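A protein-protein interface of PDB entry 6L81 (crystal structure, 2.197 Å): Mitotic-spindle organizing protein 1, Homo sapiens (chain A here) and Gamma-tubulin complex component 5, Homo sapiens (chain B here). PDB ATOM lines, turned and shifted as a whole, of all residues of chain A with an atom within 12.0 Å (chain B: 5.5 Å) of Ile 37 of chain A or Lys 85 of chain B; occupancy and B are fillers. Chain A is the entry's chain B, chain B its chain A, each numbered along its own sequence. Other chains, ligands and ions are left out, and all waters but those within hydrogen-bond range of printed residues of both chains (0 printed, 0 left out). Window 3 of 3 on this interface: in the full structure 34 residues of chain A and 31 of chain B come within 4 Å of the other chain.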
ATOM      1  N   THR A  27      34.056 -29.341   2.079  1.00  0.00           N
ATOM      2  CA  THR A  27      33.372 -28.399   2.956  1.00  0.00           C
ATOM      3  C   THR A  27      32.380 -27.537   2.180  1.00  0.00           C
ATOM      4  O   THR A  27      31.245 -27.333   2.632  1.00  0.00           O
ATOM      5  CB  THR A  27      34.371 -27.518   3.711  1.00  0.00           C
ATOM      6  OG1 THR A  27      34.832 -26.475   2.851  1.00  0.00           O
ATOM      7  CG2 THR A  27      35.534 -28.316   4.239  1.00  0.00           C
ATOM      8  N   MET A  28      32.779 -27.031   1.007  1.00  0.00           N
ATOM      9  CA  MET A  28      31.863 -26.209   0.215  1.00  0.00           C
ATOM     10  C   MET A  28      30.591 -26.969  -0.140  1.00  0.00           C
ATOM     11  O   MET A  28      29.502 -26.373  -0.182  1.00  0.00           O
ATOM     12  CB  MET A  28      32.550 -25.697  -1.052  1.00  0.00           C
ATOM     13  CG  MET A  28      33.595 -24.624  -0.765  1.00  0.00           C
ATOM     14  SD  MET A  28      32.981 -23.382   0.410  1.00  0.00           S
ATOM     15  CE  MET A  28      31.636 -22.646  -0.526  1.00  0.00           C
ATOM     16  N   ASP A  29      30.701 -28.285  -0.360  1.00  0.00           N
ATOM     17  CA  ASP A  29      29.516 -29.080  -0.676  1.00  0.00           C
ATOM     18  C   ASP A  29      28.658 -29.326   0.563  1.00  0.00           C
ATOM     19  O   ASP A  29      27.424 -29.320   0.474  1.00  0.00           O
ATOM     20  CB  ASP A  29      29.917 -30.411  -1.331  1.00  0.00           C
ATOM     21  CG  ASP A  29      30.656 -30.219  -2.666  1.00  0.00           C
ATOM     22  OD1 ASP A  29      30.625 -29.104  -3.236  1.00  0.00           O
ATOM     23  OD2 ASP A  29      31.234 -31.201  -3.166  1.00  0.00           O
ATOM     24  N   VAL A  30      29.284 -29.551   1.722  1.00  0.00           N
ATOM     25  CA  VAL A  30      28.526 -29.584   2.979  1.00  0.00           C
ATOM     26  C   VAL A  30      27.769 -28.267   3.173  1.00  0.00           C
ATOM     27  O   VAL A  30      26.556 -28.247   3.432  1.00  0.00           O
ATOM     28  CB  VAL A  30      29.469 -29.873   4.161  1.00  0.00           C
ATOM     29  CG1 VAL A  30      28.784 -29.558   5.475  1.00  0.00           C
ATOM     30  CG2 VAL A  30      29.969 -31.343   4.132  1.00  0.00           C
ATOM     31  N   LEU A  31      28.476 -27.150   3.001  1.00  0.00           N
ATOM     32  CA  LEU A  31      27.890 -25.830   3.209  1.00  0.00           C
ATOM     33  C   LEU A  31      26.739 -25.574   2.244  1.00  0.00           C
ATOM     34  O   LEU A  31      25.692 -25.037   2.637  1.00  0.00           O
ATOM     35  CB  LEU A  31      28.975 -24.768   3.044  1.00  0.00           C
ATOM     36  CG  LEU A  31      29.133 -23.657   4.074  1.00  0.00           C
ATOM     37  CD1 LEU A  31      29.026 -24.214   5.484  1.00  0.00           C
ATOM     38  CD2 LEU A  31      30.492 -22.990   3.861  1.00  0.00           C
ATOM     39  N   LEU A  32      26.904 -25.953   0.980  1.00  0.00           N
ATOM     40  CA  LEU A  32      25.818 -25.733   0.027  1.00  0.00           C
ATOM     41  C   LEU A  32      24.587 -26.546   0.399  1.00  0.00           C
ATOM     42  O   LEU A  32      23.449 -26.078   0.253  1.00  0.00           O
ATOM     43  CB  LEU A  32      26.268 -26.082  -1.396  1.00  0.00           C
ATOM     44  CG  LEU A  32      25.154 -25.825  -2.413  1.00  0.00           C
ATOM     45  CD1 LEU A  32      24.994 -24.319  -2.659  1.00  0.00           C
ATOM     46  CD2 LEU A  32      25.402 -26.579  -3.709  1.00  0.00           C
ATOM     47  N   GLU A  33      24.793 -27.771   0.877  1.00  0.00           N
ATOM     48  CA  GLU A  33      23.648 -28.550   1.316  1.00  0.00           C
ATOM     49  C   GLU A  33      23.008 -27.922   2.551  1.00  0.00           C
ATOM     50  O   GLU A  33      21.776 -27.828   2.631  1.00  0.00           O
ATOM     51  CB  GLU A  33      24.063 -29.997   1.562  1.00  0.00           C
ATOM     52  CG  GLU A  33      22.914 -30.906   1.955  1.00  0.00           C
ATOM     53  CD  GLU A  33      21.705 -30.816   1.036  1.00  0.00           C
ATOM     54  OE1 GLU A  33      21.882 -30.586  -0.179  1.00  0.00           O
ATOM     55  OE2 GLU A  33      20.572 -30.984   1.541  1.00  0.00           O
ATOM     56  N   ILE A  34      23.821 -27.451   3.510  1.00  0.00           N
ATOM     57  CA  ILE A  34      23.257 -26.717   4.642  1.00  0.00           C
ATOM     58  C   ILE A  34      22.473 -25.526   4.128  1.00  0.00           C
ATOM     59  O   ILE A  34      21.323 -25.291   4.523  1.00  0.00           O
ATOM     60  CB  ILE A  34      24.359 -26.283   5.634  1.00  0.00           C
ATOM     61  CG1 ILE A  34      24.920 -27.488   6.394  1.00  0.00           C
ATOM     62  CG2 ILE A  34      23.803 -25.264   6.640  1.00  0.00           C
ATOM     63  CD1 ILE A  34      26.207 -27.186   7.187  1.00  0.00           C
ATOM     64  N   SER A  35      23.070 -24.788   3.192  1.00  0.00           N
ATOM     65  CA  SER A  35      22.400 -23.628   2.609  1.00  0.00           C
ATOM     66  C   SER A  35      21.072 -24.006   1.949  1.00  0.00           C
ATOM     67  O   SER A  35      20.115 -23.211   1.949  1.00  0.00           O
ATOM     68  CB  SER A  35      23.327 -22.969   1.590  1.00  0.00           C
ATOM     69  OG  SER A  35      22.653 -21.932   0.910  1.00  0.00           O
ATOM     70  N   ARG A  36      21.009 -25.194   1.335  1.00  0.00           N
ATOM     71  CA  ARG A  36      19.773 -25.595   0.661  1.00  0.00           C
ATOM     72  C   ARG A  36      18.697 -25.986   1.669  1.00  0.00           C
ATOM     73  O   ARG A  36      17.529 -25.619   1.503  1.00  0.00           O
ATOM     74  CB  ARG A  36      20.045 -26.749  -0.307  1.00  0.00           C
ATOM     75  CG  ARG A  36      20.907 -26.338  -1.485  1.00  0.00           C
ATOM     76  CD  ARG A  36      20.842 -27.346  -2.623  1.00  0.00           C
ATOM     77  NE  ARG A  36      21.527 -26.844  -3.811  1.00  0.00           N
ATOM     78  CZ  ARG A  36      22.170 -27.606  -4.689  1.00  0.00           C
ATOM     79  NH1 ARG A  36      22.218 -28.924  -4.525  1.00  0.00           N
ATOM     80  NH2 ARG A  36      22.761 -27.048  -5.740  1.00  0.00           N
ATOM     81  N   ILE A  37      19.065 -26.740   2.714  1.00  0.00           N
ATOM     82  CA  ILE A  37      18.106 -27.059   3.770  1.00  0.00           C
ATOM     83  C   ILE A  37      17.505 -25.780   4.332  1.00  0.00           C
ATOM     84  O   ILE A  37      16.284 -25.663   4.484  1.00  0.00           O
ATOM     85  CB  ILE A  37      18.770 -27.910   4.868  1.00  0.00           C
ATOM     86  CG1 ILE A  37      19.182 -29.271   4.301  1.00  0.00           C
ATOM     87  CG2 ILE A  37      17.816 -28.082   6.057  1.00  0.00           C
ATOM     88  CD1 ILE A  37      19.923 -30.155   5.277  1.00  0.00           C
ATOM     89  N   LEU A  38      18.339 -24.778   4.588  1.00  0.00           N
ATOM     90  CA  LEU A  38      17.828 -23.514   5.102  1.00  0.00           C
ATOM     91  C   LEU A  38      17.114 -22.671   4.045  1.00  0.00           C
ATOM     92  O   LEU A  38      16.527 -21.646   4.407  1.00  0.00           O
ATOM     93  CB  LEU A  38      18.971 -22.691   5.735  1.00  0.00           C
ATOM     94  CG  LEU A  38      19.590 -23.268   7.018  1.00  0.00           C
ATOM     95  CD1 LEU A  38      20.899 -22.556   7.374  1.00  0.00           C
ATOM     96  CD2 LEU A  38      18.594 -23.235   8.204  1.00  0.00           C
ATOM     97  N   ASN A  39      17.154 -23.059   2.761  1.00  0.00           N
ATOM     98  CA  ASN A  39      16.439 -22.342   1.696  1.00  0.00           C
ATOM     99  C   ASN A  39      16.885 -20.876   1.616  1.00  0.00           C
ATOM    100  O   ASN A  39      16.075 -19.946   1.666  1.00  0.00           O
ATOM    101  CB  ASN A  39      14.918 -22.451   1.894  1.00  0.00           C
ATOM    102  CG  ASN A  39      14.125 -21.918   0.705  1.00  0.00           C
ATOM    103  OD1 ASN A  39      14.503 -22.127  -0.448  1.00  0.00           O
ATOM    104  ND2 ASN A  39      13.023 -21.222   0.985  1.00  0.00           N
ATOM    105  N   THR A  40      18.203 -20.667   1.523  1.00  0.00           N
ATOM    106  CA  THR A  40      18.739 -19.309   1.463  1.00  0.00           C
ATOM    107  C   THR A  40      18.666 -18.711   0.065  1.00  0.00           C
ATOM    108  O   THR A  40      18.809 -17.491  -0.084  1.00  0.00           O
ATOM    109  CB  THR A  40      20.202 -19.278   1.908  1.00  0.00           C
ATOM    110  OG1 THR A  40      20.991 -19.949   0.921  1.00  0.00           O
ATOM    111  CG2 THR A  40      20.396 -19.951   3.287  1.00  0.00           C
ATOM    112  N   GLY A  41      18.482 -19.540  -0.956  1.00  0.00           N
ATOM    113  CA  GLY A  41      18.530 -19.084  -2.325  1.00  0.00           C
ATOM    114  C   GLY A  41      19.917 -18.939  -2.906  1.00  0.00           C
ATOM    115  O   GLY A  41      20.042 -18.518  -4.061  1.00  0.00           O
ATOM    116  N   LEU A  42      20.967 -19.246  -2.150  1.00  0.00           N
ATOM    117  CA  LEU A  42      22.314 -19.086  -2.680  1.00  0.00           C
ATOM    118  C   LEU A  42      22.692 -20.250  -3.586  1.00  0.00           C
ATOM    119  O   LEU A  42      22.382 -21.414  -3.310  1.00  0.00           O
ATOM    120  CB  LEU A  42      23.355 -18.957  -1.564  1.00  0.00           C
ATOM    121  CG  LEU A  42      23.171 -17.859  -0.517  1.00  0.00           C
ATOM    122  CD1 LEU A  42      23.969 -18.149   0.700  1.00  0.00           C
ATOM    123  CD2 LEU A  42      23.573 -16.507  -1.090  1.00  0.00           C
ATOM    124  N   ASP A  43      23.362 -19.911  -4.674  1.00  0.00           N
ATOM    125  CA  ASP A  43      24.092 -20.834  -5.521  1.00  0.00           C
ATOM    126  C   ASP A  43      25.498 -21.058  -4.957  1.00  0.00           C
ATOM    127  O   ASP A  43      25.969 -20.336  -4.074  1.00  0.00           O
ATOM    128  CB  ASP A  43      24.192 -20.262  -6.931  1.00  0.00           C
ATOM    129  CG  ASP A  43      24.794 -18.871  -6.926  1.00  0.00           C
ATOM    130  OD1 ASP A  43      24.042 -17.894  -6.725  1.00  0.00           O
ATOM    131  OD2 ASP A  43      26.028 -18.760  -7.045  1.00  0.00           O
ATOM    132  N   MET A  44      26.195 -22.041  -5.526  1.00  0.00           N
ATOM    133  CA  MET A  44      27.552 -22.348  -5.083  1.00  0.00           C
ATOM    134  C   MET A  44      28.512 -21.175  -5.316  1.00  0.00           C
ATOM    135  O   MET A  44      29.417 -20.932  -4.504  1.00  0.00           O
ATOM    136  CB  MET A  44      28.053 -23.598  -5.802  1.00  0.00           C
ATOM    137  CG  MET A  44      29.482 -23.930  -5.465  1.00  0.00           C
ATOM    138  SD  MET A  44      29.647 -24.347  -3.722  1.00  0.00           S
ATOM    139  CE  MET A  44      29.321 -26.122  -3.779  1.00  0.00           C
ATOM    140  N   LEU A  47      27.725 -18.482  -2.825  1.00  0.00           N
ATOM    141  CA  LEU A  47      28.025 -19.006  -1.488  1.00  0.00           C
ATOM    142  C   LEU A  47      29.520 -18.931  -1.207  1.00  0.00           C
ATOM    143  O   LEU A  47      29.936 -18.530  -0.107  1.00  0.00           O
ATOM    144  CB  LEU A  47      27.526 -20.448  -1.329  1.00  0.00           C
ATOM    145  CG  LEU A  47      28.024 -21.169  -0.056  1.00  0.00           C
ATOM    146  CD1 LEU A  47      27.574 -20.441   1.202  1.00  0.00           C
ATOM    147  CD2 LEU A  47      27.541 -22.623   0.009  1.00  0.00           C
ATOM    148  N   PHE B  77      13.012 -30.456  12.973  1.00  0.00           N
ATOM    149  CA  PHE B  77      12.948 -31.555  12.024  1.00  0.00           C
ATOM    150  C   PHE B  77      12.454 -32.830  12.701  1.00  0.00           C
ATOM    151  O   PHE B  77      11.569 -33.516  12.174  1.00  0.00           O
ATOM    152  CB  PHE B  77      14.312 -31.763  11.365  1.00  0.00           C
ATOM    153  CG  PHE B  77      14.720 -30.642  10.434  1.00  0.00           C
ATOM    154  CD1 PHE B  77      13.759 -29.831   9.834  1.00  0.00           C
ATOM    155  CD2 PHE B  77      16.062 -30.400  10.158  1.00  0.00           C
ATOM    156  CE1 PHE B  77      14.127 -28.805   8.985  1.00  0.00           C
ATOM    157  CE2 PHE B  77      16.438 -29.366   9.307  1.00  0.00           C
ATOM    158  CZ  PHE B  77      15.479 -28.567   8.727  1.00  0.00           C
ATOM    159  N   ASP B  82      10.411 -35.539  10.110  1.00  0.00           N
ATOM    160  CA  ASP B  82      11.229 -35.528   8.894  1.00  0.00           C
ATOM    161  C   ASP B  82      12.605 -36.069   9.272  1.00  0.00           C
ATOM    162  O   ASP B  82      13.567 -35.330   9.508  1.00  0.00           O
ATOM    163  CB  ASP B  82      11.313 -34.139   8.273  1.00  0.00           C
ATOM    164  CG  ASP B  82      11.893 -34.169   6.857  1.00  0.00           C
ATOM    165  OD1 ASP B  82      12.521 -35.185   6.487  1.00  0.00           O
ATOM    166  OD2 ASP B  82      11.724 -33.180   6.112  1.00  0.00           O
ATOM    167  N   LEU B  83      12.679 -37.402   9.317  1.00  0.00           N
ATOM    168  CA  LEU B  83      13.863 -38.085   9.823  1.00  0.00           C
ATOM    169  C   LEU B  83      15.052 -37.936   8.879  1.00  0.00           C
ATOM    170  O   LEU B  83      16.183 -37.736   9.331  1.00  0.00           O
ATOM    171  CB  LEU B  83      13.539 -39.559  10.056  1.00  0.00           C
ATOM    172  CG  LEU B  83      13.150 -39.965  11.482  1.00  0.00           C
ATOM    173  CD1 LEU B  83      14.398 -40.170  12.319  1.00  0.00           C
ATOM    174  CD2 LEU B  83      12.252 -38.917  12.126  1.00  0.00           C
ATOM    175  N   SER B  84      14.822 -38.041   7.566  1.00  0.00           N
ATOM    176  CA  SER B  84      15.931 -37.927   6.627  1.00  0.00           C
ATOM    177  C   SER B  84      16.464 -36.502   6.549  1.00  0.00           C
ATOM    178  O   SER B  84      17.609 -36.303   6.130  1.00  0.00           O
ATOM    179  CB  SER B  84      15.519 -38.408   5.231  1.00  0.00           C
ATOM    180  OG  SER B  84      14.711 -37.448   4.566  1.00  0.00           O
ATOM    181  N   LYS B  85      15.668 -35.510   6.945  1.00  0.00           N
ATOM    182  CA  LYS B  85      16.192 -34.152   7.015  1.00  0.00           C
ATOM    183  C   LYS B  85      16.884 -33.877   8.343  1.00  0.00           C
ATOM    184  O   LYS B  85      17.899 -33.179   8.365  1.00  0.00           O
ATOM    185  CB  LYS B  85      15.082 -33.126   6.781  1.00  0.00           C
ATOM    186  CG  LYS B  85      15.579 -31.873   6.075  1.00  0.00           C
ATOM    187  CD  LYS B  85      14.482 -30.831   5.917  1.00  0.00           C
ATOM    188  CE  LYS B  85      14.810 -29.852   4.789  1.00  0.00           C
ATOM    189  NZ  LYS B  85      13.899 -28.663   4.751  1.00  0.00           N
ATOM    190  N   ALA B  86      16.371 -34.431   9.448  1.00  0.00           N
ATOM    191  CA  ALA B  86      17.019 -34.239  10.740  1.00  0.00           C
ATOM    192  C   ALA B  86      18.398 -34.888  10.760  1.00  0.00           C
ATOM    193  O   ALA B  86      19.387 -34.261  11.164  1.00  0.00           O
ATOM    194  CB  ALA B  86      16.147 -34.803  11.858  1.00  0.00           C
ATOM    195  N   ALA B  87      18.476 -36.156  10.328  1.00  0.00           N
ATOM    196  CA  ALA B  87      19.758 -36.854  10.277  1.00  0.00           C
ATOM    197  C   ALA B  87      20.731 -36.151   9.338  1.00  0.00           C
ATOM    198  O   ALA B  87      21.932 -36.092   9.617  1.00  0.00           O
ATOM    199  CB  ALA B  87      19.556 -38.315   9.853  1.00  0.00           C
ATOM    200  N   SER B  88      20.230 -35.608   8.220  1.00  0.00           N
ATOM    201  CA  SER B  88      21.085 -34.850   7.312  1.00  0.00           C
ATOM    202  C   SER B  88      21.572 -33.569   7.974  1.00  0.00           C
ATOM    203  O   SER B  88      22.772 -33.255   7.941  1.00  0.00           O
ATOM    204  CB  SER B  88      20.340 -34.520   6.019  1.00  0.00           C
ATOM    205  OG  SER B  88      20.221 -35.654   5.188  1.00  0.00           O
ATOM    206  N   TRP B  89      20.643 -32.817   8.574  1.00  0.00           N
ATOM    207  CA  TRP B  89      20.984 -31.586   9.278  1.00  0.00           C
ATOM    208  C   TRP B  89      22.077 -31.817  10.313  1.00  0.00           C
ATOM    209  O   TRP B  89      23.107 -31.139  10.303  1.00  0.00           O
ATOM    210  CB  TRP B  89      19.751 -31.015   9.961  1.00  0.00           C
ATOM    211  CG  TRP B  89      20.064 -29.767  10.721  1.00  0.00           C
ATOM    212  CD1 TRP B  89      20.125 -29.619  12.072  1.00  0.00           C
ATOM    213  CD2 TRP B  89      20.365 -28.489  10.160  1.00  0.00           C
ATOM    214  NE1 TRP B  89      20.439 -28.320  12.387  1.00  0.00           N
ATOM    215  CE2 TRP B  89      20.598 -27.608  11.230  1.00  0.00           C
ATOM    216  CE3 TRP B  89      20.443 -27.999   8.854  1.00  0.00           C
ATOM    217  CZ2 TRP B  89      20.898 -26.251  11.037  1.00  0.00           C
ATOM    218  CZ3 TRP B  89      20.751 -26.652   8.662  1.00  0.00           C
ATOM    219  CH2 TRP B  89      20.973 -25.798   9.749  1.00  0.00           C
ATOM    220  N   LYS B  90      21.861 -32.781  11.214  1.00  0.00           N
ATOM    221  CA  LYS B  90      22.857 -33.049  12.236  1.00  0.00           C
ATOM    222  C   LYS B  90      24.180 -33.483  11.613  1.00  0.00           C
ATOM    223  O   LYS B  90      25.247 -33.044  12.054  1.00  0.00           O
ATOM    224  CB  LYS B  90      22.352 -34.107  13.220  1.00  0.00           C
ATOM    225  CG  LYS B  90      23.479 -34.655  14.099  1.00  0.00           C
ATOM    226  CD  LYS B  90      23.046 -35.806  15.003  1.00  0.00           C
ATOM    227  CE  LYS B  90      22.392 -35.277  16.264  1.00  0.00           C
ATOM    228  NZ  LYS B  90      22.344 -36.296  17.352  1.00  0.00           N
ATOM    229  N   LEU B  92      25.499 -32.835   8.559  1.00  0.00           N
ATOM    230  CA  LEU B  92      26.217 -31.773   7.857  1.00  0.00           C
ATOM    231  C   LEU B  92      26.791 -30.744   8.825  1.00  0.00           C
ATOM    232  O   LEU B  92      27.953 -30.348   8.702  1.00  0.00           O
ATOM    233  CB  LEU B  92      25.295 -31.084   6.854  1.00  0.00           C
ATOM    234  CG  LEU B  92      24.853 -32.015   5.727  1.00  0.00           C
ATOM    235  CD1 LEU B  92      23.491 -31.588   5.251  1.00  0.00           C
ATOM    236  CD2 LEU B  92      25.883 -32.009   4.595  1.00  0.00           C
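Of chain B, only Phe 77 (3.6 Å), Lys 85 (3.7 Å), Trp 89 (3.8 Å) and Leu 92 (3.8 Å) come within 4 Å of Ile 37 of chain A. Lys 85 of chain B touches one residue of chain A. Phe 77 of chain B touches one residue of chain A. No residue of chain A comes within 4 Å of Asp 82 of chain B. No residue of chain A comes within 4 Å of Leu 83 of chain B. Ala 86 of chain B touches none of the printed residues of chain A. No residue of chain A comes within 4 Å of Ser 88 of chain B. Printed residues of chain A within 4 Å of Trp 89 of chain B: Ile 34 (3.9 Å), Ile 37 (3.8 Å) and Leu 38 (3.8 Å). Of the printed residues of chain B, Val 30 of chain A touches Leu 92 (3.4 Å). Printed residues of chain B within 4 Å of Glu 33 of chain A: Leu 92 (3.4 Å). Printed residues of chain B within 4 Å of Leu 38 of chain A: Trp 89 (3.8 Å). Of the printed residues of chain B, Ile 34 of chain A touches Trp 89 and Leu 92. Printed residues of chain A within 4 Å of Leu 92 of chain B: Val 30 (3.4 Å), Glu 33 (3.4 Å), Ile 34 (3.6 Å) and Ile 37 (3.8 Å). The nearest printed residue of chain B that does not touch Leu 38 of chain A is Lys 85 of chain B (5.9 Å).
The backbone NH of Asp 82 of chain B sits at hydrogen-bond distance from the backbone carbonyl oxygen of Phe 77 of chain B, 3.1 Å away. The side-chain carboxylate of Asp 82 of chain B sits at hydrogen-bond distance from the backbone NH of Lys 85 of chain B, at 3.2 Å.
Of the 11 printed residues of chain B, 4 touch a printed residue of chain A. Hydrophobic or aromatic side chains of chain B that line the printed part of chain A: Phe 77, Trp 89 and Leu 92. Of the 19 printed residues of chain A, 5 touch a printed residue of chain B. Printed residues of chain A that touch a printed residue of chain B: Val 30, Glu 33, Ile 34, Ile 37 and Leu 38. Hydrophobic or aromatic side chains of chain A that line the printed part of chain B: Val 30, Ile 34, Ile 37 and Leu 38.
O of Leu 92 of chain B touches CG1 of Val 30 of chain A (3.4 Å). Glu 33 of chain A touches Leu 92 of chain B. Ile 34 of chain A touches Trp 89 of chain B. CB of Leu 92 of chain B touches CG1 of Ile 34 of chain A, at 3.6 Å. Ile 37 of chain A touches Phe 77 of chain B. Ile 37 of chain A touches Lys 85 of chain B. Trp 89 of chain B touches Ile 37 of chain A. Leu 92 of chain B touches Ile 37 of chain A (CD1 to CD1, 3.8 Å). Leu 38 of chain A touches Trp 89 of chain B (CD2 to CH2, 3.8 Å).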
